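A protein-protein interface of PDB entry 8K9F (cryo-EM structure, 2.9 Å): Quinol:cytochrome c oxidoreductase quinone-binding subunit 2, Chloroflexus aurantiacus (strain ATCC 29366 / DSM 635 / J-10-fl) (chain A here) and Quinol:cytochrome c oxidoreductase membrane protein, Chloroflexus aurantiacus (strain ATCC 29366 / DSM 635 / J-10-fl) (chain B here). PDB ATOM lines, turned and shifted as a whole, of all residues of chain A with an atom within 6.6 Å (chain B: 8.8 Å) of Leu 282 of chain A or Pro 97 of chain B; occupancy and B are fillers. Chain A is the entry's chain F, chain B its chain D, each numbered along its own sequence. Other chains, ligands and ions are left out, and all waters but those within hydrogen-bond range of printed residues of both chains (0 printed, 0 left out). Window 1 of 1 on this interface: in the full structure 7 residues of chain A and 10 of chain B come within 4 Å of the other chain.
The guanidinium group (NH1) of Arg 89 of chain B lies within hydrogen-bond range of the backbone carbonyl oxygen (O) of Ser 287 of chain A. OH of Tyr 279 of chain A is in hydrogen-bond range of N of Ala 98 of chain B, at 3.3 Å.
O of Pro 90 of chain B sits close to ND2 of Asn 95 of chain B (3.5 Å). The side-chain carboxylate of Asp 92 of chain B lies close to the backbone NH of Thr 94 of chain B (3.4 Å). The backbone NH (N) of Leu 282 of chain A sits at hydrogen-bond distance from the side-chain hydroxyl (OH) of Tyr 297 of chain A (3.3 Å). The backbone carbonyl oxygen of Val 283 of chain A sits close to the side-chain hydroxyl of Ser 287 of chain A (3.3 Å).
Of chain B, only Trp 96 and Pro 97 come within 4 Å of Leu 282 of chain A. Of chain A, only Leu 282 (3.7 Å) and Trp 286 (3.4 Å) come within 4 Å of Pro 97 of chain B. No residue of chain B comes within 4 Å of Gly 280 of chain A. Of the printed residues of chain A, Pro 90 of chain B touches Trp 286. Printed residues of chain B within 4 Å of Trp 286 of chain A: Arg 89 (3.9 Å), Pro 90 (3.9 Å), Thr 94 (3.8 Å), Asn 95 (3.4 Å) and Pro 97 (3.4 Å). Printed residues of chain A within 4 Å of Trp 96 of chain B: Leu 282 and Met 313. The nearest residue of chain B that does not touch Leu 282 of chain A is Ala 98 of chain B (6.7 Å). The nearest printed residue of chain A that does not touch Asn 95 of chain B is Ser 287 of chain A (7.3 Å).
Among the printed residues, pairs that only touch across the chains: Tyr 279 of chain A with Ile 100 of chain B (3.5 Å), Tyr 279 of chain A with Pro 101 of chain B (3.2 Å), Leu 282 of chain A with Trp 96 of chain B (3.6 Å), Leu 282 of chain A with Pro 97 of chain B (3.7 Å), Val 283 of chain A with Ala 98 of chain B (3.9 Å), Trp 286 of chain A with Arg 89 of chain B (3.9 Å), Trp 286 of chain A with Pro 90 of chain B (3.9 Å), Trp 286 of chain A with Thr 94 of chain B (3.8 Å), Trp 286 of chain A with Asn 95 of chain B (3.4 Å), Trp 286 of chain A with Pro 97 of chain B (3.4 Å) and Met 313 of chain A with Trp 96 of chain B (3.5 Å).
Of the 14 printed residues of chain A, 6 touch a printed residue of chain B. Hydrophobic or aromatic side chains of chain B that line the printed part of chain A: Pro 90, Trp 96, Pro 97, Ile 100 and Pro 101. Along chain B the printed residues that touch a printed residue of chain A span positions 89 to 101. Among the printed residues, 13 pairs touch across the chains.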
ATOM      1  N   MET A 277       9.727 -16.421  23.794  1.00  0.00           N
ATOM      2  CA  MET A 277       8.890 -15.401  23.162  1.00  0.00           C
ATOM      3  C   MET A 277       9.313 -13.991  23.563  1.00  0.00           C
ATOM      4  O   MET A 277       9.430 -13.098  22.706  1.00  0.00           O
ATOM      5  CB  MET A 277       7.432 -15.655  23.536  1.00  0.00           C
ATOM      6  CG  MET A 277       6.432 -15.283  22.481  1.00  0.00           C
ATOM      7  SD  MET A 277       6.057 -16.688  21.425  1.00  0.00           S
ATOM      8  CE  MET A 277       5.671 -17.937  22.639  1.00  0.00           C
ATOM      9  N   SER A 278       9.561 -13.780  24.859  1.00  0.00           N
ATOM     10  CA  SER A 278       9.979 -12.471  25.348  1.00  0.00           C
ATOM     11  C   SER A 278      11.362 -12.094  24.842  1.00  0.00           C
ATOM     12  O   SER A 278      11.588 -10.940  24.462  1.00  0.00           O
ATOM     13  CB  SER A 278       9.953 -12.439  26.870  1.00  0.00           C
ATOM     14  OG  SER A 278       8.634 -12.578  27.325  1.00  0.00           O
ATOM     15  N   TYR A 279      12.297 -13.050  24.817  1.00  0.00           N
ATOM     16  CA  TYR A 279      13.604 -12.764  24.247  1.00  0.00           C
ATOM     17  C   TYR A 279      13.521 -12.527  22.751  1.00  0.00           C
ATOM     18  O   TYR A 279      14.294 -11.729  22.224  1.00  0.00           O
ATOM     19  CB  TYR A 279      14.596 -13.891  24.529  1.00  0.00           C
ATOM     20  CG  TYR A 279      15.949 -13.591  23.934  1.00  0.00           C
ATOM     21  CD1 TYR A 279      16.756 -12.612  24.491  1.00  0.00           C
ATOM     22  CD2 TYR A 279      16.390 -14.231  22.781  1.00  0.00           C
ATOM     23  CE1 TYR A 279      17.975 -12.309  23.947  1.00  0.00           C
ATOM     24  CE2 TYR A 279      17.604 -13.925  22.223  1.00  0.00           C
ATOM     25  CZ  TYR A 279      18.394 -12.966  22.815  1.00  0.00           C
ATOM     26  OH  TYR A 279      19.615 -12.653  22.278  1.00  0.00           O
ATOM     27  N   GLY A 280      12.612 -13.216  22.055  1.00  0.00           N
ATOM     28  CA  GLY A 280      12.459 -12.986  20.629  1.00  0.00           C
ATOM     29  C   GLY A 280      12.009 -11.575  20.326  1.00  0.00           C
ATOM     30  O   GLY A 280      12.632 -10.879  19.523  1.00  0.00           O
ATOM     31  N   GLN A 281      10.979 -11.107  21.041  1.00  0.00           N
ATOM     32  CA  GLN A 281      10.523  -9.727  20.884  1.00  0.00           C
ATOM     33  C   GLN A 281      11.603  -8.732  21.279  1.00  0.00           C
ATOM     34  O   GLN A 281      11.818  -7.725  20.587  1.00  0.00           O
ATOM     35  CB  GLN A 281       9.281  -9.486  21.729  1.00  0.00           C
ATOM     36  CG  GLN A 281       8.603  -8.164  21.440  1.00  0.00           C
ATOM     37  CD  GLN A 281       7.630  -7.766  22.523  1.00  0.00           C
ATOM     38  OE1 GLN A 281       7.698  -6.663  23.055  1.00  0.00           O
ATOM     39  NE2 GLN A 281       6.707  -8.660  22.846  1.00  0.00           N
ATOM     40  N   LEU A 282      12.312  -9.025  22.373  1.00  0.00           N
ATOM     41  CA  LEU A 282      13.331  -8.123  22.882  1.00  0.00           C
ATOM     42  C   LEU A 282      14.501  -8.002  21.920  1.00  0.00           C
ATOM     43  O   LEU A 282      14.937  -6.893  21.623  1.00  0.00           O
ATOM     44  CB  LEU A 282      13.800  -8.610  24.246  1.00  0.00           C
ATOM     45  CG  LEU A 282      14.765  -7.720  25.011  1.00  0.00           C
ATOM     46  CD1 LEU A 282      14.267  -7.559  26.434  1.00  0.00           C
ATOM     47  CD2 LEU A 282      16.131  -8.329  24.994  1.00  0.00           C
ATOM     48  N   VAL A 283      15.003  -9.120  21.398  1.00  0.00           N
ATOM     49  CA  VAL A 283      16.173  -9.056  20.536  1.00  0.00           C
ATOM     50  C   VAL A 283      15.798  -8.551  19.148  1.00  0.00           C
ATOM     51  O   VAL A 283      16.635  -7.941  18.471  1.00  0.00           O
ATOM     52  CB  VAL A 283      16.899 -10.418  20.501  1.00  0.00           C
ATOM     53  CG1 VAL A 283      16.220 -11.415  19.583  1.00  0.00           C
ATOM     54  CG2 VAL A 283      18.361 -10.243  20.108  1.00  0.00           C
ATOM     55  N   ILE A 284      14.537  -8.720  18.728  1.00  0.00           N
ATOM     56  CA  ILE A 284      14.108  -8.173  17.445  1.00  0.00           C
ATOM     57  C   ILE A 284      14.022  -6.659  17.519  1.00  0.00           C
ATOM     58  O   ILE A 284      14.553  -5.948  16.657  1.00  0.00           O
ATOM     59  CB  ILE A 284      12.768  -8.798  17.027  1.00  0.00           C
ATOM     60  CG1 ILE A 284      13.013 -10.168  16.426  1.00  0.00           C
ATOM     61  CG2 ILE A 284      12.016  -7.925  16.027  1.00  0.00           C
ATOM     62  CD1 ILE A 284      11.780 -10.977  16.318  1.00  0.00           C
ATOM     63  N   ILE A 285      13.367  -6.142  18.558  1.00  0.00           N
ATOM     64  CA  ILE A 285      13.210  -4.702  18.682  1.00  0.00           C
ATOM     65  C   ILE A 285      14.535  -4.048  19.070  1.00  0.00           C
ATOM     66  O   ILE A 285      14.880  -2.965  18.581  1.00  0.00           O
ATOM     67  CB  ILE A 285      12.072  -4.410  19.676  1.00  0.00           C
ATOM     68  CG1 ILE A 285      10.743  -4.816  19.035  1.00  0.00           C
ATOM     69  CG2 ILE A 285      12.046  -2.967  20.077  1.00  0.00           C
ATOM     70  CD1 ILE A 285       9.559  -4.821  19.959  1.00  0.00           C
ATOM     71  N   TRP A 286      15.327  -4.727  19.899  1.00  0.00           N
ATOM     72  CA  TRP A 286      16.577  -4.172  20.396  1.00  0.00           C
ATOM     73  C   TRP A 286      17.644  -4.141  19.317  1.00  0.00           C
ATOM     74  O   TRP A 286      18.353  -3.142  19.169  1.00  0.00           O
ATOM     75  CB  TRP A 286      17.043  -4.987  21.601  1.00  0.00           C
ATOM     76  CG  TRP A 286      18.252  -4.457  22.288  1.00  0.00           C
ATOM     77  CD1 TRP A 286      18.284  -3.577  23.319  1.00  0.00           C
ATOM     78  CD2 TRP A 286      19.611  -4.805  22.012  1.00  0.00           C
ATOM     79  NE1 TRP A 286      19.578  -3.341  23.698  1.00  0.00           N
ATOM     80  CE2 TRP A 286      20.414  -4.083  22.907  1.00  0.00           C
ATOM     81  CE3 TRP A 286      20.226  -5.649  21.085  1.00  0.00           C
ATOM     82  CZ2 TRP A 286      21.800  -4.178  22.909  1.00  0.00           C
ATOM     83  CZ3 TRP A 286      21.599  -5.743  21.087  1.00  0.00           C
ATOM     84  CH2 TRP A 286      22.372  -5.013  21.992  1.00  0.00           C
ATOM     85  N   SER A 287      17.784  -5.226  18.552  1.00  0.00           N
ATOM     86  CA  SER A 287      18.815  -5.246  17.524  1.00  0.00           C
ATOM     87  C   SER A 287      18.428  -4.380  16.331  1.00  0.00           C
ATOM     88  O   SER A 287      19.259  -3.629  15.811  1.00  0.00           O
ATOM     89  CB  SER A 287      19.097  -6.677  17.095  1.00  0.00           C
ATOM     90  OG  SER A 287      19.876  -7.346  18.068  1.00  0.00           O
ATOM     91  N   TYR A 297      10.243  -0.470  24.932  1.00  0.00           N
ATOM     92  CA  TYR A 297      11.335  -0.828  25.821  1.00  0.00           C
ATOM     93  C   TYR A 297      12.036   0.375  26.415  1.00  0.00           C
ATOM     94  O   TYR A 297      12.784   0.218  27.381  1.00  0.00           O
ATOM     95  CB  TYR A 297      12.363  -1.689  25.096  1.00  0.00           C
ATOM     96  CG  TYR A 297      11.860  -3.068  24.802  1.00  0.00           C
ATOM     97  CD1 TYR A 297      11.861  -4.051  25.780  1.00  0.00           C
ATOM     98  CD2 TYR A 297      11.362  -3.384  23.556  1.00  0.00           C
ATOM     99  CE1 TYR A 297      11.394  -5.316  25.510  1.00  0.00           C
ATOM    100  CE2 TYR A 297      10.896  -4.637  23.278  1.00  0.00           C
ATOM    101  CZ  TYR A 297      10.911  -5.602  24.254  1.00  0.00           C
ATOM    102  OH  TYR A 297      10.435  -6.858  23.964  1.00  0.00           O
ATOM    103  N   MET A 313      13.706 -11.465  34.806  1.00  0.00           N
ATOM    104  CA  MET A 313      14.626 -12.377  34.138  1.00  0.00           C
ATOM    105  C   MET A 313      15.278 -13.346  35.117  1.00  0.00           C
ATOM    106  O   MET A 313      15.552 -14.496  34.760  1.00  0.00           O
ATOM    107  CB  MET A 313      15.675 -11.560  33.397  1.00  0.00           C
ATOM    108  CG  MET A 313      15.089 -10.903  32.182  1.00  0.00           C
ATOM    109  SD  MET A 313      16.240  -9.934  31.227  1.00  0.00           S
ATOM    110  CE  MET A 313      15.104  -8.699  30.588  1.00  0.00           C
ATOM    111  N   TRP A 353       4.795  -5.703  34.659  1.00  0.00           N
ATOM    112  CA  TRP A 353       5.766  -5.123  33.723  1.00  0.00           C
ATOM    113  C   TRP A 353       5.192  -4.940  32.319  1.00  0.00           C
ATOM    114  O   TRP A 353       5.654  -4.081  31.565  1.00  0.00           O
ATOM    115  CB  TRP A 353       7.018  -5.998  33.655  1.00  0.00           C
ATOM    116  CG  TRP A 353       8.140  -5.428  32.840  1.00  0.00           C
ATOM    117  CD1 TRP A 353       8.980  -4.411  33.187  1.00  0.00           C
ATOM    118  CD2 TRP A 353       8.535  -5.842  31.531  1.00  0.00           C
ATOM    119  NE1 TRP A 353       9.880  -4.175  32.180  1.00  0.00           N
ATOM    120  CE2 TRP A 353       9.630  -5.043  31.152  1.00  0.00           C
ATOM    121  CE3 TRP A 353       8.076  -6.816  30.645  1.00  0.00           C
ATOM    122  CZ2 TRP A 353      10.263  -5.182  29.920  1.00  0.00           C
ATOM    123  CZ3 TRP A 353       8.709  -6.956  29.426  1.00  0.00           C
ATOM    124  CH2 TRP A 353       9.788  -6.143  29.074  1.00  0.00           C
ATOM    125  N   PHE B  71      29.352 -17.499  26.846  1.00  0.00           N
ATOM    126  CA  PHE B  71      29.201 -16.135  27.339  1.00  0.00           C
ATOM    127  C   PHE B  71      30.547 -15.449  27.536  1.00  0.00           C
ATOM    128  O   PHE B  71      30.737 -14.306  27.098  1.00  0.00           O
ATOM    129  CB  PHE B  71      28.413 -16.150  28.647  1.00  0.00           C
ATOM    130  CG  PHE B  71      28.469 -14.861  29.401  1.00  0.00           C
ATOM    131  CD1 PHE B  71      27.774 -13.751  28.960  1.00  0.00           C
ATOM    132  CD2 PHE B  71      29.211 -14.763  30.571  1.00  0.00           C
ATOM    133  CE1 PHE B  71      27.825 -12.567  29.666  1.00  0.00           C
ATOM    134  CE2 PHE B  71      29.271 -13.578  31.272  1.00  0.00           C
ATOM    135  CZ  PHE B  71      28.576 -12.480  30.817  1.00  0.00           C
ATOM    136  N   GLN B  74      32.195 -14.704  24.067  1.00  0.00           N
ATOM    137  CA  GLN B  74      31.646 -13.506  23.434  1.00  0.00           C
ATOM    138  C   GLN B  74      32.106 -12.234  24.138  1.00  0.00           C
ATOM    139  O   GLN B  74      32.473 -11.255  23.474  1.00  0.00           O
ATOM    140  CB  GLN B  74      30.123 -13.555  23.413  1.00  0.00           C
ATOM    141  CG  GLN B  74      29.540 -14.633  22.554  1.00  0.00           C
ATOM    142  CD  GLN B  74      28.040 -14.560  22.510  1.00  0.00           C
ATOM    143  OE1 GLN B  74      27.470 -13.849  21.687  1.00  0.00           O
ATOM    144  NE2 GLN B  74      27.384 -15.286  23.405  1.00  0.00           N
ATOM    145  N   LEU B  79      34.187  -7.488  23.601  1.00  0.00           N
ATOM    146  CA  LEU B  79      34.128  -6.366  24.519  1.00  0.00           C
ATOM    147  C   LEU B  79      35.414  -6.119  25.290  1.00  0.00           C
ATOM    148  O   LEU B  79      35.547  -5.052  25.897  1.00  0.00           O
ATOM    149  CB  LEU B  79      32.963  -6.540  25.510  1.00  0.00           C
ATOM    150  CG  LEU B  79      31.588  -6.900  24.933  1.00  0.00           C
ATOM    151  CD1 LEU B  79      30.534  -6.990  26.019  1.00  0.00           C
ATOM    152  CD2 LEU B  79      31.140  -5.911  23.882  1.00  0.00           C
ATOM    153  N   ARG B  89      26.114  -0.373  19.173  1.00  0.00           N
ATOM    154  CA  ARG B  89      25.809  -1.336  20.214  1.00  0.00           C
ATOM    155  C   ARG B  89      26.739  -1.112  21.402  1.00  0.00           C
ATOM    156  O   ARG B  89      27.863  -0.636  21.228  1.00  0.00           O
ATOM    157  CB  ARG B  89      25.967  -2.760  19.683  1.00  0.00           C
ATOM    158  CG  ARG B  89      25.278  -3.026  18.365  1.00  0.00           C
ATOM    159  CD  ARG B  89      23.814  -2.680  18.396  1.00  0.00           C
ATOM    160  NE  ARG B  89      23.436  -1.749  17.341  1.00  0.00           N
ATOM    161  CZ  ARG B  89      22.317  -1.834  16.634  1.00  0.00           C
ATOM    162  NH1 ARG B  89      21.445  -2.807  16.835  1.00  0.00           N
ATOM    163  NH2 ARG B  89      22.073  -0.926  15.694  1.00  0.00           N
ATOM    164  N   PRO B  90      26.284  -1.403  22.621  1.00  0.00           N
ATOM    165  CA  PRO B  90      27.113  -1.111  23.794  1.00  0.00           C
ATOM    166  C   PRO B  90      28.289  -2.066  23.915  1.00  0.00           C
ATOM    167  O   PRO B  90      28.295  -3.173  23.374  1.00  0.00           O
ATOM    168  CB  PRO B  90      26.142  -1.267  24.966  1.00  0.00           C
ATOM    169  CG  PRO B  90      25.071  -2.145  24.462  1.00  0.00           C
ATOM    170  CD  PRO B  90      24.939  -1.867  23.010  1.00  0.00           C
ATOM    171  N   ASP B  92      29.497  -2.975  26.999  1.00  0.00           N
ATOM    172  CA  ASP B  92      29.455  -3.449  28.375  1.00  0.00           C
ATOM    173  C   ASP B  92      28.426  -4.567  28.506  1.00  0.00           C
ATOM    174  O   ASP B  92      27.998  -5.135  27.501  1.00  0.00           O
ATOM    175  CB  ASP B  92      29.172  -2.294  29.344  1.00  0.00           C
ATOM    176  CG  ASP B  92      27.858  -1.574  29.061  1.00  0.00           C
ATOM    177  OD1 ASP B  92      27.249  -1.785  27.995  1.00  0.00           O
ATOM    178  OD2 ASP B  92      27.428  -0.780  29.926  1.00  0.00           O
ATOM    179  N   ILE B  93      28.042  -4.902  29.741  1.00  0.00           N
ATOM    180  CA  ILE B  93      27.080  -5.972  29.990  1.00  0.00           C
ATOM    181  C   ILE B  93      25.674  -5.657  29.494  1.00  0.00           C
ATOM    182  O   ILE B  93      24.848  -6.568  29.393  1.00  0.00           O
ATOM    183  CB  ILE B  93      27.069  -6.306  31.498  1.00  0.00           C
ATOM    184  CG1 ILE B  93      26.736  -7.785  31.730  1.00  0.00           C
ATOM    185  CG2 ILE B  93      26.127  -5.386  32.260  1.00  0.00           C
ATOM    186  CD1 ILE B  93      27.739  -8.734  31.108  1.00  0.00           C
ATOM    187  N   THR B  94      25.386  -4.399  29.137  1.00  0.00           N
ATOM    188  CA  THR B  94      24.107  -4.023  28.548  1.00  0.00           C
ATOM    189  C   THR B  94      23.945  -4.546  27.126  1.00  0.00           C
ATOM    190  O   THR B  94      22.850  -4.457  26.564  1.00  0.00           O
ATOM    191  CB  THR B  94      23.961  -2.501  28.577  1.00  0.00           C
ATOM    192  OG1 THR B  94      23.995  -2.059  29.935  1.00  0.00           O
ATOM    193  CG2 THR B  94      22.640  -2.072  27.971  1.00  0.00           C
ATOM    194  N   ASN B  95      25.010  -5.096  26.543  1.00  0.00           N
ATOM    195  CA  ASN B  95      25.007  -5.813  25.281  1.00  0.00           C
ATOM    196  C   ASN B  95      24.634  -7.297  25.529  1.00  0.00           C
ATOM    197  O   ASN B  95      24.969  -8.175  24.729  1.00  0.00           O
ATOM    198  CB  ASN B  95      26.399  -5.574  24.635  1.00  0.00           C
ATOM    199  CG  ASN B  95      26.556  -5.992  23.152  1.00  0.00           C
ATOM    200  OD1 ASN B  95      25.585  -5.935  22.405  1.00  0.00           O
ATOM    201  ND2 ASN B  95      27.707  -6.534  22.776  1.00  0.00           N
ATOM    202  N   TRP B  96      23.969  -7.597  26.655  1.00  0.00           N
ATOM    203  CA  TRP B  96      23.463  -8.939  26.930  1.00  0.00           C
ATOM    204  C   TRP B  96      22.490  -9.472  25.864  1.00  0.00           C
ATOM    205  O   TRP B  96      22.604 -10.663  25.553  1.00  0.00           O
ATOM    206  CB  TRP B  96      22.866  -9.028  28.353  1.00  0.00           C
ATOM    207  CG  TRP B  96      21.537  -8.403  28.550  1.00  0.00           C
ATOM    208  CD1 TRP B  96      21.282  -7.128  28.954  1.00  0.00           C
ATOM    209  CD2 TRP B  96      20.266  -9.009  28.307  1.00  0.00           C
ATOM    210  NE1 TRP B  96      19.931  -6.903  28.985  1.00  0.00           N
ATOM    211  CE2 TRP B  96      19.285  -8.042  28.584  1.00  0.00           C
ATOM    212  CE3 TRP B  96      19.865 -10.270  27.861  1.00  0.00           C
ATOM    213  CZ2 TRP B  96      17.932  -8.302  28.449  1.00  0.00           C
ATOM    214  CZ3 TRP B  96      18.522 -10.528  27.727  1.00  0.00           C
ATOM    215  CH2 TRP B  96      17.571  -9.550  28.018  1.00  0.00           C
ATOM    216  N   PRO B  97      21.555  -8.716  25.253  1.00  0.00           N
ATOM    217  CA  PRO B  97      20.920  -9.279  24.055  1.00  0.00           C
ATOM    218  C   PRO B  97      21.933  -9.219  22.925  1.00  0.00           C
ATOM    219  O   PRO B  97      22.809  -8.351  22.928  1.00  0.00           O
ATOM    220  CB  PRO B  97      19.722  -8.356  23.797  1.00  0.00           C
ATOM    221  CG  PRO B  97      19.683  -7.417  24.921  1.00  0.00           C
ATOM    222  CD  PRO B  97      21.054  -7.331  25.417  1.00  0.00           C
ATOM    223  N   ALA B  98      21.811 -10.155  21.980  1.00  0.00           N
ATOM    224  CA  ALA B  98      22.816 -10.519  20.979  1.00  0.00           C
ATOM    225  C   ALA B  98      24.063 -11.090  21.643  1.00  0.00           C
ATOM    226  O   ALA B  98      25.171 -10.962  21.119  1.00  0.00           O
ATOM    227  CB  ALA B  98      23.183  -9.357  20.036  1.00  0.00           C
ATOM    228  N   MET B  99      23.886 -11.717  22.798  1.00  0.00           N
ATOM    229  CA  MET B  99      24.890 -12.597  23.370  1.00  0.00           C
ATOM    230  C   MET B  99      24.305 -13.888  23.916  1.00  0.00           C
ATOM    231  O   MET B  99      25.054 -14.835  24.159  1.00  0.00           O
ATOM    232  CB  MET B  99      25.676 -11.862  24.462  1.00  0.00           C
ATOM    233  CG  MET B  99      27.071 -11.481  23.998  1.00  0.00           C
ATOM    234  SD  MET B  99      27.905 -10.249  25.006  1.00  0.00           S
ATOM    235  CE  MET B  99      27.440 -10.796  26.624  1.00  0.00           C
ATOM    236  N   ILE B 100      22.990 -13.943  24.106  1.00  0.00           N
ATOM    237  CA  ILE B 100      22.235 -15.130  24.519  1.00  0.00           C
ATOM    238  C   ILE B 100      22.272 -16.298  23.523  1.00  0.00           C
ATOM    239  O   ILE B 100      22.434 -17.438  23.994  1.00  0.00           O
ATOM    240  CB  ILE B 100      20.787 -14.730  24.896  1.00  0.00           C
ATOM    241  CG1 ILE B 100      20.648 -14.538  26.407  1.00  0.00           C
ATOM    242  CG2 ILE B 100      19.737 -15.765  24.486  1.00  0.00           C
ATOM    243  CD1 ILE B 100      21.421 -13.395  26.987  1.00  0.00           C
ATOM    244  N   PRO B 101      22.117 -16.134  22.189  1.00  0.00           N
ATOM    245  CA  PRO B 101      22.022 -17.344  21.344  1.00  0.00           C
ATOM    246  C   PRO B 101      23.304 -18.149  21.236  1.00  0.00           C
ATOM    247  O   PRO B 101      23.236 -19.380  21.198  1.00  0.00           O
ATOM    248  CB  PRO B 101      21.608 -16.785  19.976  1.00  0.00           C
ATOM    249  CG  PRO B 101      22.021 -15.400  20.004  1.00  0.00           C
ATOM    250  CD  PRO B 101      21.711 -14.966  21.379  1.00  0.00           C
